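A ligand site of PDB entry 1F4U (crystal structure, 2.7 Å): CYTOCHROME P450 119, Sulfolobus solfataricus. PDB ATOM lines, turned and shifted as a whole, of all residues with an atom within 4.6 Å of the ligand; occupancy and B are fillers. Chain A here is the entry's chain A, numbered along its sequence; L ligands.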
ATOM      1  N   LEU A  33      29.770  -9.098  23.951  1.00  0.00           N
ATOM      2  CA  LEU A  33      28.646  -8.478  24.671  1.00  0.00           C
ATOM      3  C   LEU A  33      29.034  -7.712  25.949  1.00  0.00           C
ATOM      4  O   LEU A  33      28.412  -6.700  26.268  1.00  0.00           O
ATOM      5  CB  LEU A  33      27.604  -9.541  25.030  1.00  0.00           C
ATOM      6  CG  LEU A  33      26.712 -10.197  23.979  1.00  0.00           C
ATOM      7  CD1 LEU A  33      25.879 -11.311  24.630  1.00  0.00           C
ATOM      8  CD2 LEU A  33      25.805  -9.158  23.353  1.00  0.00           C
ATOM      9  N   MET A  68      17.805   3.535  25.103  1.00  0.00           N
ATOM     10  CA  MET A  68      18.985   2.955  25.744  1.00  0.00           C
ATOM     11  C   MET A  68      19.549   1.735  25.021  1.00  0.00           C
ATOM     12  O   MET A  68      20.748   1.510  25.019  1.00  0.00           O
ATOM     13  CB  MET A  68      18.656   2.594  27.195  1.00  0.00           C
ATOM     14  CG  MET A  68      17.728   1.422  27.336  1.00  0.00           C
ATOM     15  SD  MET A  68      17.226   1.195  29.031  1.00  0.00           S
ATOM     16  CE  MET A  68      15.600   0.600  28.842  1.00  0.00           C
ATOM     17  N   LEU A  69      18.667   0.955  24.405  1.00  0.00           N
ATOM     18  CA  LEU A  69      19.057  -0.252  23.691  1.00  0.00           C
ATOM     19  C   LEU A  69      20.136   0.030  22.662  1.00  0.00           C
ATOM     20  O   LEU A  69      20.969  -0.810  22.373  1.00  0.00           O
ATOM     21  CB  LEU A  69      17.846  -0.858  22.990  1.00  0.00           C
ATOM     22  CG  LEU A  69      18.052  -2.196  22.263  1.00  0.00           C
ATOM     23  CD1 LEU A  69      18.530  -3.247  23.254  1.00  0.00           C
ATOM     24  CD2 LEU A  69      16.736  -2.628  21.631  1.00  0.00           C
ATOM     25  N   HIS A  76      23.895   5.514  28.333  1.00  0.00           N
ATOM     26  CA  HIS A  76      23.191   4.297  28.717  1.00  0.00           C
ATOM     27  C   HIS A  76      22.751   4.262  30.183  1.00  0.00           C
ATOM     28  O   HIS A  76      21.553   4.147  30.488  1.00  0.00           O
ATOM     29  CB  HIS A  76      24.055   3.071  28.434  1.00  0.00           C
ATOM     30  CG  HIS A  76      23.424   1.781  28.852  1.00  0.00           C
ATOM     31  ND1 HIS A  76      22.231   1.347  28.331  1.00  0.00           N
ATOM     32  CD2 HIS A  76      23.771   0.897  29.812  1.00  0.00           C
ATOM     33  CE1 HIS A  76      21.853   0.248  28.953  1.00  0.00           C
ATOM     34  NE2 HIS A  76      22.770  -0.048  29.856  1.00  0.00           N
ATOM     35  N   ARG A  80      18.952   4.137  31.878  1.00  0.00           N
ATOM     36  CA  ARG A  80      18.465   2.957  32.579  1.00  0.00           C
ATOM     37  C   ARG A  80      18.074   3.215  34.035  1.00  0.00           C
ATOM     38  O   ARG A  80      17.167   2.562  34.544  1.00  0.00           O
ATOM     39  CB  ARG A  80      19.488   1.830  32.510  1.00  0.00           C
ATOM     40  CG  ARG A  80      18.949   0.500  33.010  1.00  0.00           C
ATOM     41  CD  ARG A  80      19.726  -0.631  32.419  1.00  0.00           C
ATOM     42  NE  ARG A  80      19.167  -1.912  32.807  1.00  0.00           N
ATOM     43  CZ  ARG A  80      19.473  -3.077  32.231  1.00  0.00           C
ATOM     44  NH1 ARG A  80      20.322  -3.117  31.213  1.00  0.00           N
ATOM     45  NH2 ARG A  80      18.906  -4.190  32.654  1.00  0.00           N
ATOM     46  N   PHE A  87      11.391  -2.709  37.316  1.00  0.00           N
ATOM     47  CA  PHE A  87      11.193  -4.069  36.821  1.00  0.00           C
ATOM     48  C   PHE A  87      11.870  -5.118  37.691  1.00  0.00           C
ATOM     49  O   PHE A  87      11.617  -6.312  37.536  1.00  0.00           O
ATOM     50  CB  PHE A  87      11.681  -4.188  35.371  1.00  0.00           C
ATOM     51  CG  PHE A  87      10.846  -3.428  34.396  1.00  0.00           C
ATOM     52  CD1 PHE A  87      10.973  -2.037  34.272  1.00  0.00           C
ATOM     53  CD2 PHE A  87       9.890  -4.088  33.618  1.00  0.00           C
ATOM     54  CE1 PHE A  87      10.152  -1.320  33.419  1.00  0.00           C
ATOM     55  CE2 PHE A  87       9.062  -3.380  32.758  1.00  0.00           C
ATOM     56  CZ  PHE A  87       9.193  -1.993  32.647  1.00  0.00           C
ATOM     57  N   ILE A 130       1.794  -5.493  30.205  1.00  0.00           N
ATOM     58  CA  ILE A 130       2.657  -4.334  30.036  1.00  0.00           C
ATOM     59  C   ILE A 130       1.823  -3.075  30.110  1.00  0.00           C
ATOM     60  O   ILE A 130       2.271  -2.037  30.583  1.00  0.00           O
ATOM     61  CB  ILE A 130       3.435  -4.358  28.702  1.00  0.00           C
ATOM     62  CG1 ILE A 130       4.468  -3.241  28.702  1.00  0.00           C
ATOM     63  CG2 ILE A 130       2.501  -4.187  27.530  1.00  0.00           C
ATOM     64  CD1 ILE A 130       5.478  -3.362  29.814  1.00  0.00           C
ATOM     65  N   LEU A 155      16.796  -6.650  17.280  1.00  0.00           N
ATOM     66  CA  LEU A 155      18.250  -6.624  17.455  1.00  0.00           C
ATOM     67  C   LEU A 155      19.186  -6.877  16.273  1.00  0.00           C
ATOM     68  O   LEU A 155      20.239  -7.490  16.444  1.00  0.00           O
ATOM     69  CB  LEU A 155      18.602  -7.592  18.601  1.00  0.00           C
ATOM     70  CG  LEU A 155      17.595  -7.529  19.747  1.00  0.00           C
ATOM     71  CD1 LEU A 155      17.837  -8.659  20.740  1.00  0.00           C
ATOM     72  CD2 LEU A 155      17.689  -6.145  20.399  1.00  0.00           C
ATOM     73  N   LEU A 205       9.549   1.845  23.553  1.00  0.00           N
ATOM     74  CA  LEU A 205      10.382   0.700  23.888  1.00  0.00           C
ATOM     75  C   LEU A 205       9.758  -0.161  24.979  1.00  0.00           C
ATOM     76  O   LEU A 205       9.445  -1.326  24.767  1.00  0.00           O
ATOM     77  CB  LEU A 205      11.765   1.181  24.348  1.00  0.00           C
ATOM     78  CG  LEU A 205      12.786   0.147  24.798  1.00  0.00           C
ATOM     79  CD1 LEU A 205      13.184  -0.742  23.636  1.00  0.00           C
ATOM     80  CD2 LEU A 205      14.013   0.850  25.317  1.00  0.00           C
ATOM     81  N   LEU A 206       9.580   0.421  26.155  1.00  0.00           N
ATOM     82  CA  LEU A 206       8.989  -0.294  27.268  1.00  0.00           C
ATOM     83  C   LEU A 206       7.633  -0.900  26.931  1.00  0.00           C
ATOM     84  O   LEU A 206       7.264  -1.917  27.492  1.00  0.00           O
ATOM     85  CB  LEU A 206       8.812   0.652  28.460  1.00  0.00           C
ATOM     86  CG  LEU A 206      10.055   1.370  28.970  1.00  0.00           C
ATOM     87  CD1 LEU A 206       9.672   2.366  30.060  1.00  0.00           C
ATOM     88  CD2 LEU A 206      11.049   0.353  29.495  1.00  0.00           C
ATOM     89  N   ALA A 209       8.813  -3.356  22.885  1.00  0.00           N
ATOM     90  CA  ALA A 209       9.992  -4.204  22.882  1.00  0.00           C
ATOM     91  C   ALA A 209       9.822  -5.674  23.261  1.00  0.00           C
ATOM     92  O   ALA A 209      10.190  -6.550  22.480  1.00  0.00           O
ATOM     93  CB  ALA A 209      11.081  -3.580  23.750  1.00  0.00           C
ATOM     94  N   GLY A 210       9.284  -5.959  24.442  1.00  0.00           N
ATOM     95  CA  GLY A 210       9.153  -7.343  24.874  1.00  0.00           C
ATOM     96  C   GLY A 210       7.876  -8.154  24.669  1.00  0.00           C
ATOM     97  O   GLY A 210       7.775  -9.266  25.193  1.00  0.00           O
ATOM     98  N   THR A 213       8.791 -11.074  21.845  1.00  0.00           N
ATOM     99  CA  THR A 213       9.713 -12.034  22.461  1.00  0.00           C
ATOM    100  C   THR A 213       9.050 -12.872  23.562  1.00  0.00           C
ATOM    101  O   THR A 213       9.153 -14.093  23.548  1.00  0.00           O
ATOM    102  CB  THR A 213      10.963 -11.346  23.045  1.00  0.00           C
ATOM    103  OG1 THR A 213      10.600 -10.043  23.512  1.00  0.00           O
ATOM    104  CG2 THR A 213      12.055 -11.219  22.013  1.00  0.00           C
ATOM    105  N   THR A 214       8.370 -12.229  24.511  1.00  0.00           N
ATOM    106  CA  THR A 214       7.715 -12.992  25.574  1.00  0.00           C
ATOM    107  C   THR A 214       6.634 -13.945  25.015  1.00  0.00           C
ATOM    108  O   THR A 214       6.402 -15.028  25.552  1.00  0.00           O
ATOM    109  CB  THR A 214       7.085 -12.063  26.618  1.00  0.00           C
ATOM    110  OG1 THR A 214       8.054 -11.111  27.046  1.00  0.00           O
ATOM    111  CG2 THR A 214       6.606 -12.860  27.819  1.00  0.00           C
ATOM    112  N   LEU A 217       8.482 -16.915  23.751  1.00  0.00           N
ATOM    113  CA  LEU A 217       8.986 -17.754  24.822  1.00  0.00           C
ATOM    114  C   LEU A 217       7.898 -18.737  25.246  1.00  0.00           C
ATOM    115  O   LEU A 217       8.116 -19.952  25.270  1.00  0.00           O
ATOM    116  CB  LEU A 217       9.414 -16.897  26.024  1.00  0.00           C
ATOM    117  CG  LEU A 217       9.970 -17.662  27.232  1.00  0.00           C
ATOM    118  CD1 LEU A 217      11.108 -18.586  26.811  1.00  0.00           C
ATOM    119  CD2 LEU A 217      10.442 -16.655  28.263  1.00  0.00           C
ATOM    120  N   LEU A 248      14.606 -21.176  27.307  1.00  0.00           N
ATOM    121  CA  LEU A 248      15.307 -19.984  26.865  1.00  0.00           C
ATOM    122  C   LEU A 248      16.640 -20.341  26.220  1.00  0.00           C
ATOM    123  O   LEU A 248      17.040 -19.713  25.235  1.00  0.00           O
ATOM    124  CB  LEU A 248      15.555 -19.033  28.044  1.00  0.00           C
ATOM    125  CG  LEU A 248      14.370 -18.222  28.576  1.00  0.00           C
ATOM    126  CD1 LEU A 248      14.754 -17.553  29.864  1.00  0.00           C
ATOM    127  CD2 LEU A 248      13.953 -17.183  27.554  1.00  0.00           C
ATOM    128  N   PRO A 253      14.267 -16.859  21.822  1.00  0.00           N
ATOM    129  CA  PRO A 253      13.376 -16.034  20.995  1.00  0.00           C
ATOM    130  C   PRO A 253      14.147 -15.262  19.925  1.00  0.00           C
ATOM    131  O   PRO A 253      13.735 -15.205  18.771  1.00  0.00           O
ATOM    132  CB  PRO A 253      12.716 -15.112  22.009  1.00  0.00           C
ATOM    133  CG  PRO A 253      12.619 -15.988  23.215  1.00  0.00           C
ATOM    134  CD  PRO A 253      13.999 -16.639  23.258  1.00  0.00           C
ATOM    135  N   THR A 257      22.482 -10.781  18.092  1.00  0.00           N
ATOM    136  CA  THR A 257      22.477  -9.338  18.263  1.00  0.00           C
ATOM    137  C   THR A 257      23.671  -8.848  17.489  1.00  0.00           C
ATOM    138  O   THR A 257      24.472  -9.636  17.000  1.00  0.00           O
ATOM    139  CB  THR A 257      22.676  -8.833  19.691  1.00  0.00           C
ATOM    140  OG1 THR A 257      22.096  -9.739  20.633  1.00  0.00           O
ATOM    141  CG2 THR A 257      22.003  -7.488  19.845  1.00  0.00           C
ATOM    142  N   ARG A 259      26.814  -5.682  17.195  1.00  0.00           N
ATOM    143  CA  ARG A 259      27.608  -4.681  17.871  1.00  0.00           C
ATOM    144  C   ARG A 259      28.468  -4.105  16.763  1.00  0.00           C
ATOM    145  O   ARG A 259      28.549  -4.693  15.665  1.00  0.00           O
ATOM    146  CB  ARG A 259      28.494  -5.321  18.964  1.00  0.00           C
ATOM    147  CG  ARG A 259      27.744  -5.839  20.186  1.00  0.00           C
ATOM    148  CD  ARG A 259      27.341  -4.721  21.097  1.00  0.00           C
ATOM    149  NE  ARG A 259      26.759  -5.163  22.363  1.00  0.00           N
ATOM    150  CZ  ARG A 259      25.474  -5.484  22.535  1.00  0.00           C
ATOM    151  NH1 ARG A 259      24.622  -5.422  21.532  1.00  0.00           N
ATOM    152  NH2 ARG A 259      25.035  -5.835  23.743  1.00  0.00           N
ATOM    153  N   ILE A 282      23.759 -15.651  19.700  1.00  0.00           N
ATOM    154  CA  ILE A 282      23.359 -16.115  21.029  1.00  0.00           C
ATOM    155  C   ILE A 282      22.990 -17.595  20.970  1.00  0.00           C
ATOM    156  O   ILE A 282      23.461 -18.386  21.779  1.00  0.00           O
ATOM    157  CB  ILE A 282      22.126 -15.285  21.544  1.00  0.00           C
ATOM    158  CG1 ILE A 282      22.584 -13.899  22.019  1.00  0.00           C
ATOM    159  CG2 ILE A 282      21.365 -16.041  22.637  1.00  0.00           C
ATOM    160  CD1 ILE A 282      21.436 -12.964  22.285  1.00  0.00           C
ATOM    161  N   SER A 309      20.492 -15.863  26.351  1.00  0.00           N
ATOM    162  CA  SER A 309      19.268 -15.435  25.668  1.00  0.00           C
ATOM    163  C   SER A 309      18.753 -14.053  26.037  1.00  0.00           C
ATOM    164  O   SER A 309      17.998 -13.436  25.275  1.00  0.00           O
ATOM    165  CB  SER A 309      18.161 -16.448  25.892  1.00  0.00           C
ATOM    166  OG  SER A 309      18.466 -17.686  25.277  1.00  0.00           O
ATOM    167  N   PHE A 310      19.150 -13.572  27.215  1.00  0.00           N
ATOM    168  CA  PHE A 310      18.736 -12.259  27.694  1.00  0.00           C
ATOM    169  C   PHE A 310      19.855 -11.258  27.554  1.00  0.00           C
ATOM    170  O   PHE A 310      19.730 -10.098  27.915  1.00  0.00           O
ATOM    171  CB  PHE A 310      18.318 -12.323  29.161  1.00  0.00           C
ATOM    172  CG  PHE A 310      16.921 -12.821  29.376  1.00  0.00           C
ATOM    173  CD1 PHE A 310      15.840 -12.161  28.804  1.00  0.00           C
ATOM    174  CD2 PHE A 310      16.694 -13.918  30.183  1.00  0.00           C
ATOM    175  CE1 PHE A 310      14.542 -12.598  29.045  1.00  0.00           C
ATOM    176  CE2 PHE A 310      15.401 -14.358  30.437  1.00  0.00           C
ATOM    177  CZ  PHE A 310      14.311 -13.698  29.862  1.00  0.00           C
ATOM    178  N   GLY A 311      20.980 -11.711  27.026  1.00  0.00           N
ATOM    179  CA  GLY A 311      22.087 -10.812  26.867  1.00  0.00           C
ATOM    180  C   GLY A 311      23.075 -11.062  27.979  1.00  0.00           C
ATOM    181  O   GLY A 311      22.993 -12.065  28.683  1.00  0.00           O
ATOM    182  N   ILE A 314      26.140  -4.708  30.570  1.00  0.00           N
ATOM    183  CA  ILE A 314      25.330  -3.535  30.922  1.00  0.00           C
ATOM    184  C   ILE A 314      23.969  -3.470  30.223  1.00  0.00           C
ATOM    185  O   ILE A 314      23.061  -2.812  30.702  1.00  0.00           O
ATOM    186  CB  ILE A 314      26.062  -2.219  30.613  1.00  0.00           C
ATOM    187  CG1 ILE A 314      26.153  -2.003  29.102  1.00  0.00           C
ATOM    188  CG2 ILE A 314      27.456  -2.258  31.207  1.00  0.00           C
ATOM    189  CD1 ILE A 314      26.948  -0.786  28.695  1.00  0.00           C
ATOM    190  N   HIS A 315      23.834  -4.153  29.084  1.00  0.00           N
ATOM    191  CA  HIS A 315      22.572  -4.162  28.326  1.00  0.00           C
ATOM    192  C   HIS A 315      21.664  -5.355  28.625  1.00  0.00           C
ATOM    193  O   HIS A 315      20.646  -5.521  27.961  1.00  0.00           O
ATOM    194  CB  HIS A 315      22.852  -4.108  26.820  1.00  0.00           C
ATOM    195  CG  HIS A 315      23.280  -2.762  26.316  1.00  0.00           C
ATOM    196  ND1 HIS A 315      22.473  -1.648  26.362  1.00  0.00           N
ATOM    197  CD2 HIS A 315      24.442  -2.352  25.732  1.00  0.00           C
ATOM    198  CE1 HIS A 315      23.101  -0.619  25.822  1.00  0.00           C
ATOM    199  NE2 HIS A 315      24.299  -1.017  25.435  1.00  0.00           N
ATOM    200  N   LEU A 316      22.026  -6.188  29.599  1.00  0.00           N
ATOM    201  CA  LEU A 316      21.223  -7.365  29.935  1.00  0.00           C
ATOM    202  C   LEU A 316      19.764  -6.972  29.981  1.00  0.00           C
ATOM    203  O   LEU A 316      19.410  -6.009  30.648  1.00  0.00           O
ATOM    204  CB  LEU A 316      21.637  -7.930  31.284  1.00  0.00           C
ATOM    205  CG  LEU A 316      20.735  -9.039  31.806  1.00  0.00           C
ATOM    206  CD1 LEU A 316      21.151 -10.356  31.195  1.00  0.00           C
ATOM    207  CD2 LEU A 316      20.825  -9.090  33.317  1.00  0.00           C
ATOM    208  N   CYS A 317      18.907  -7.718  29.295  1.00  0.00           N
ATOM    209  CA  CYS A 317      17.476  -7.402  29.222  1.00  0.00           C
ATOM    210  C   CYS A 317      16.868  -6.769  30.465  1.00  0.00           C
ATOM    211  O   CYS A 317      16.756  -7.399  31.504  1.00  0.00           O
ATOM    212  CB  CYS A 317      16.666  -8.647  28.840  1.00  0.00           C
ATOM    213  SG  CYS A 317      14.900  -8.274  28.458  1.00  0.00           S
ATOM    214  N   LEU A 318      16.449  -5.511  30.329  1.00  0.00           N
ATOM    215  CA  LEU A 318      15.818  -4.775  31.420  1.00  0.00           C
ATOM    216  C   LEU A 318      14.556  -5.495  31.897  1.00  0.00           C
ATOM    217  O   LEU A 318      14.155  -5.340  33.049  1.00  0.00           O
ATOM    218  CB  LEU A 318      15.421  -3.358  30.961  1.00  0.00           C
ATOM    219  CG  LEU A 318      14.695  -2.483  31.995  1.00  0.00           C
ATOM    220  CD1 LEU A 318      15.618  -2.202  33.161  1.00  0.00           C
ATOM    221  CD2 LEU A 318      14.283  -1.170  31.372  1.00  0.00           C
ATOM    222  N   GLY A 319      13.953  -6.295  31.027  1.00  0.00           N
ATOM    223  CA  GLY A 319      12.723  -6.985  31.377  1.00  0.00           C
ATOM    224  C   GLY A 319      12.835  -8.488  31.584  1.00  0.00           C
ATOM    225  O   GLY A 319      11.813  -9.194  31.515  1.00  0.00           O
ATOM    226  N   ALA A 323       9.710 -11.185  32.011  1.00  0.00           N
ATOM    227  CA  ALA A 323       9.490 -12.227  31.016  1.00  0.00           C
ATOM    228  C   ALA A 323       9.420 -13.572  31.743  1.00  0.00           C
ATOM    229  O   ALA A 323       8.534 -14.389  31.479  1.00  0.00           O
ATOM    230  CB  ALA A 323      10.636 -12.226  30.013  1.00  0.00           C
HETATM  231  C1  LIG L   1      17.353  -5.986  25.976  1.00  0.00           C
HETATM  232  C2  LIG L   1      15.884 -10.584  25.087  1.00  0.00           C
HETATM  233  C3  LIG L   1      11.629  -9.675  27.150  1.00  0.00           C
HETATM  234  C4  LIG L   1      12.770  -4.977  27.370  1.00  0.00           C
HETATM  235  C5  LIG L   1      17.371  -7.377  25.629  1.00  0.00           C
HETATM  236  C6  LIG L   1      18.510  -8.109  25.054  1.00  0.00           C
HETATM  237  C7  LIG L   1      18.043  -9.383  24.770  1.00  0.00           C
HETATM  238  C8  LIG L   1      16.632  -9.405  25.116  1.00  0.00           C
HETATM  239  C9  LIG L   1      18.811 -10.607  24.282  1.00  0.00           C
HETATM  240  C10 LIG L   1      19.934  -7.625  24.789  1.00  0.00           C
HETATM  241  C11 LIG L   1      20.295  -6.708  23.617  1.00  0.00           C
HETATM  242  C12 LIG L   1      21.806  -6.491  23.490  1.00  0.00           C
HETATM  243  O1  LIG L   1      22.556  -6.752  24.473  1.00  0.00           O
HETATM  244  O2  LIG L   1      22.269  -6.057  22.408  1.00  0.00           O
HETATM  245  C13 LIG L   1      14.598 -10.729  25.561  1.00  0.00           C
HETATM  246  C14 LIG L   1      13.821 -11.971  25.589  1.00  0.00           C
HETATM  247  C15 LIG L   1      12.631 -11.701  26.135  1.00  0.00           C
HETATM  248  C16 LIG L   1      12.671 -10.307  26.501  1.00  0.00           C
HETATM  249  C17 LIG L   1      14.260 -13.332  25.106  1.00  0.00           C
HETATM  250  C18 LIG L   1      11.528 -12.528  26.264  1.00  0.00           C
HETATM  251  C19 LIG L   1      11.539 -13.920  26.684  1.00  0.00           C
HETATM  252  C20 LIG L   1      11.606  -8.332  27.441  1.00  0.00           C
HETATM  253  C21 LIG L   1      10.436  -7.678  28.054  1.00  0.00           C
HETATM  254  C22 LIG L   1      10.746  -6.356  28.120  1.00  0.00           C
HETATM  255  C23 LIG L   1      12.076  -6.194  27.498  1.00  0.00           C
HETATM  256  C24 LIG L   1       9.191  -8.366  28.647  1.00  0.00           C
HETATM  257  C25 LIG L   1      10.063  -5.505  28.966  1.00  0.00           C
HETATM  258  C26 LIG L   1       9.838  -4.096  28.737  1.00  0.00           C
HETATM  259  C27 LIG L   1      14.108  -4.829  26.948  1.00  0.00           C
HETATM  260  C28 LIG L   1      14.823  -3.579  27.081  1.00  0.00           C
HETATM  261  C29 LIG L   1      16.110  -3.826  26.760  1.00  0.00           C
HETATM  262  C30 LIG L   1      16.200  -5.277  26.405  1.00  0.00           C
HETATM  263  C31 LIG L   1      14.244  -2.216  27.444  1.00  0.00           C
HETATM  264  C32 LIG L   1      17.203  -2.754  26.799  1.00  0.00           C
HETATM  265  C33 LIG L   1      18.287  -3.087  27.812  1.00  0.00           C
HETATM  266  C34 LIG L   1      19.419  -2.085  27.822  1.00  0.00           C
HETATM  267  O3  LIG L   1      19.829  -1.626  26.733  1.00  0.00           O
HETATM  268  O4  LIG L   1      19.910  -1.769  28.930  1.00  0.00           O
HETATM  269  N1  LIG L   1      16.221  -8.192  25.655  1.00  0.00           N
HETATM  270  N2  LIG L   1      13.871  -9.687  26.122  1.00  0.00           N
HETATM  271  N3  LIG L   1      12.624  -7.433  27.128  1.00  0.00           N
HETATM  272  N4  LIG L   1      14.947  -5.876  26.539  1.00  0.00           N
HETATM  273 FE1  LIG L   1      14.440  -7.779  26.336  1.00  0.00          FE
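An iron atom (FE1) of the ligand is bound by the side-chain sulfur (SG) of Cys 317, 2.2 Å away. The guanidinium group of Arg 259 is in salt-bridge range of an oxygen (O2) of the ligand, at 2.6 Å. ND1 of His 315 is in hydrogen-bond range of O3 of the ligand. O4 of the ligand lies within salt-bridge range of NH1 of Arg 80 (2.7 Å). A ring nitrogen (NE2) of His 76 sits close to an oxygen (O4) of the ligand, at 3.5 Å.
CE of Met 68 touches C31 of the ligand, at 3.4 Å. CA of Leu 69 touches O3 of the ligand, at 3.4 Å. Leu 205 touches the ligand (CD2 to C31, 3.7 Å). O of Leu 206 touches C26 of the ligand, at 3.6 Å. CA of Gly 210 touches C21 of the ligand, at 3.4 Å. CB of Thr 213 touches C18 of the ligand, at 3.5 Å. Thr 214 touches the ligand (OG1 to C24, 3.4 Å). CD2 of Leu 217 touches C19 of the ligand, at 3.3 Å. CG of Pro 253 touches C17 of the ligand, at 3.7 Å. Thr 257 touches the ligand. Ser 309 touches the ligand (O to C9, 3.1 Å). Phe 310 touches the ligand. Gly 311 touches the ligand. Ile 314 touches the ligand. CB of Leu 318 touches C31 of the ligand, 3.9 Å away. Gly 319 touches the ligand. CB of Ala 323 touches C19 of the ligand, 3.8 Å away. Hydrophobic or aromatic side chains that line the ligand: Met 68, Leu 69, His 76, Leu 205, Leu 217, Pro 253, Phe 310, His 315, Leu 318 and Ala 323. The nearest printed residue that does not touch the ligand is Ile 282 (4.1 Å).
The backbone NH (N) of Cys 317 sits at hydrogen-bond distance from the backbone carbonyl oxygen (O) of Phe 310, 2.9 Å away. The side-chain sulfur (SG) of Cys 317 sits close to the backbone NH (N) of Gly 319 (3.4 Å). NH1 of Arg 80 is in hydrogen-bond range of O of Ile 314, at 2.8 Å. The guanidinium group (NH2) of Arg 80 lies within hydrogen-bond range of the backbone carbonyl oxygen (O) of Leu 316, 2.8 Å away. NE2 of His 76 is in hydrogen-bond range of O of Ile 314, 2.9 Å away. The backbone carbonyl oxygen of Leu 248 lies within hydrogen-bond range of the side-chain hydroxyl of Ser 309 (2.5 Å). The side-chain hydroxyl of Thr 214 lies within hydrogen-bond range of the backbone carbonyl oxygen of Gly 210, 2.6 Å away. OG1 of Thr 213 sits close to O of Gly 210 (3.4 Å).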
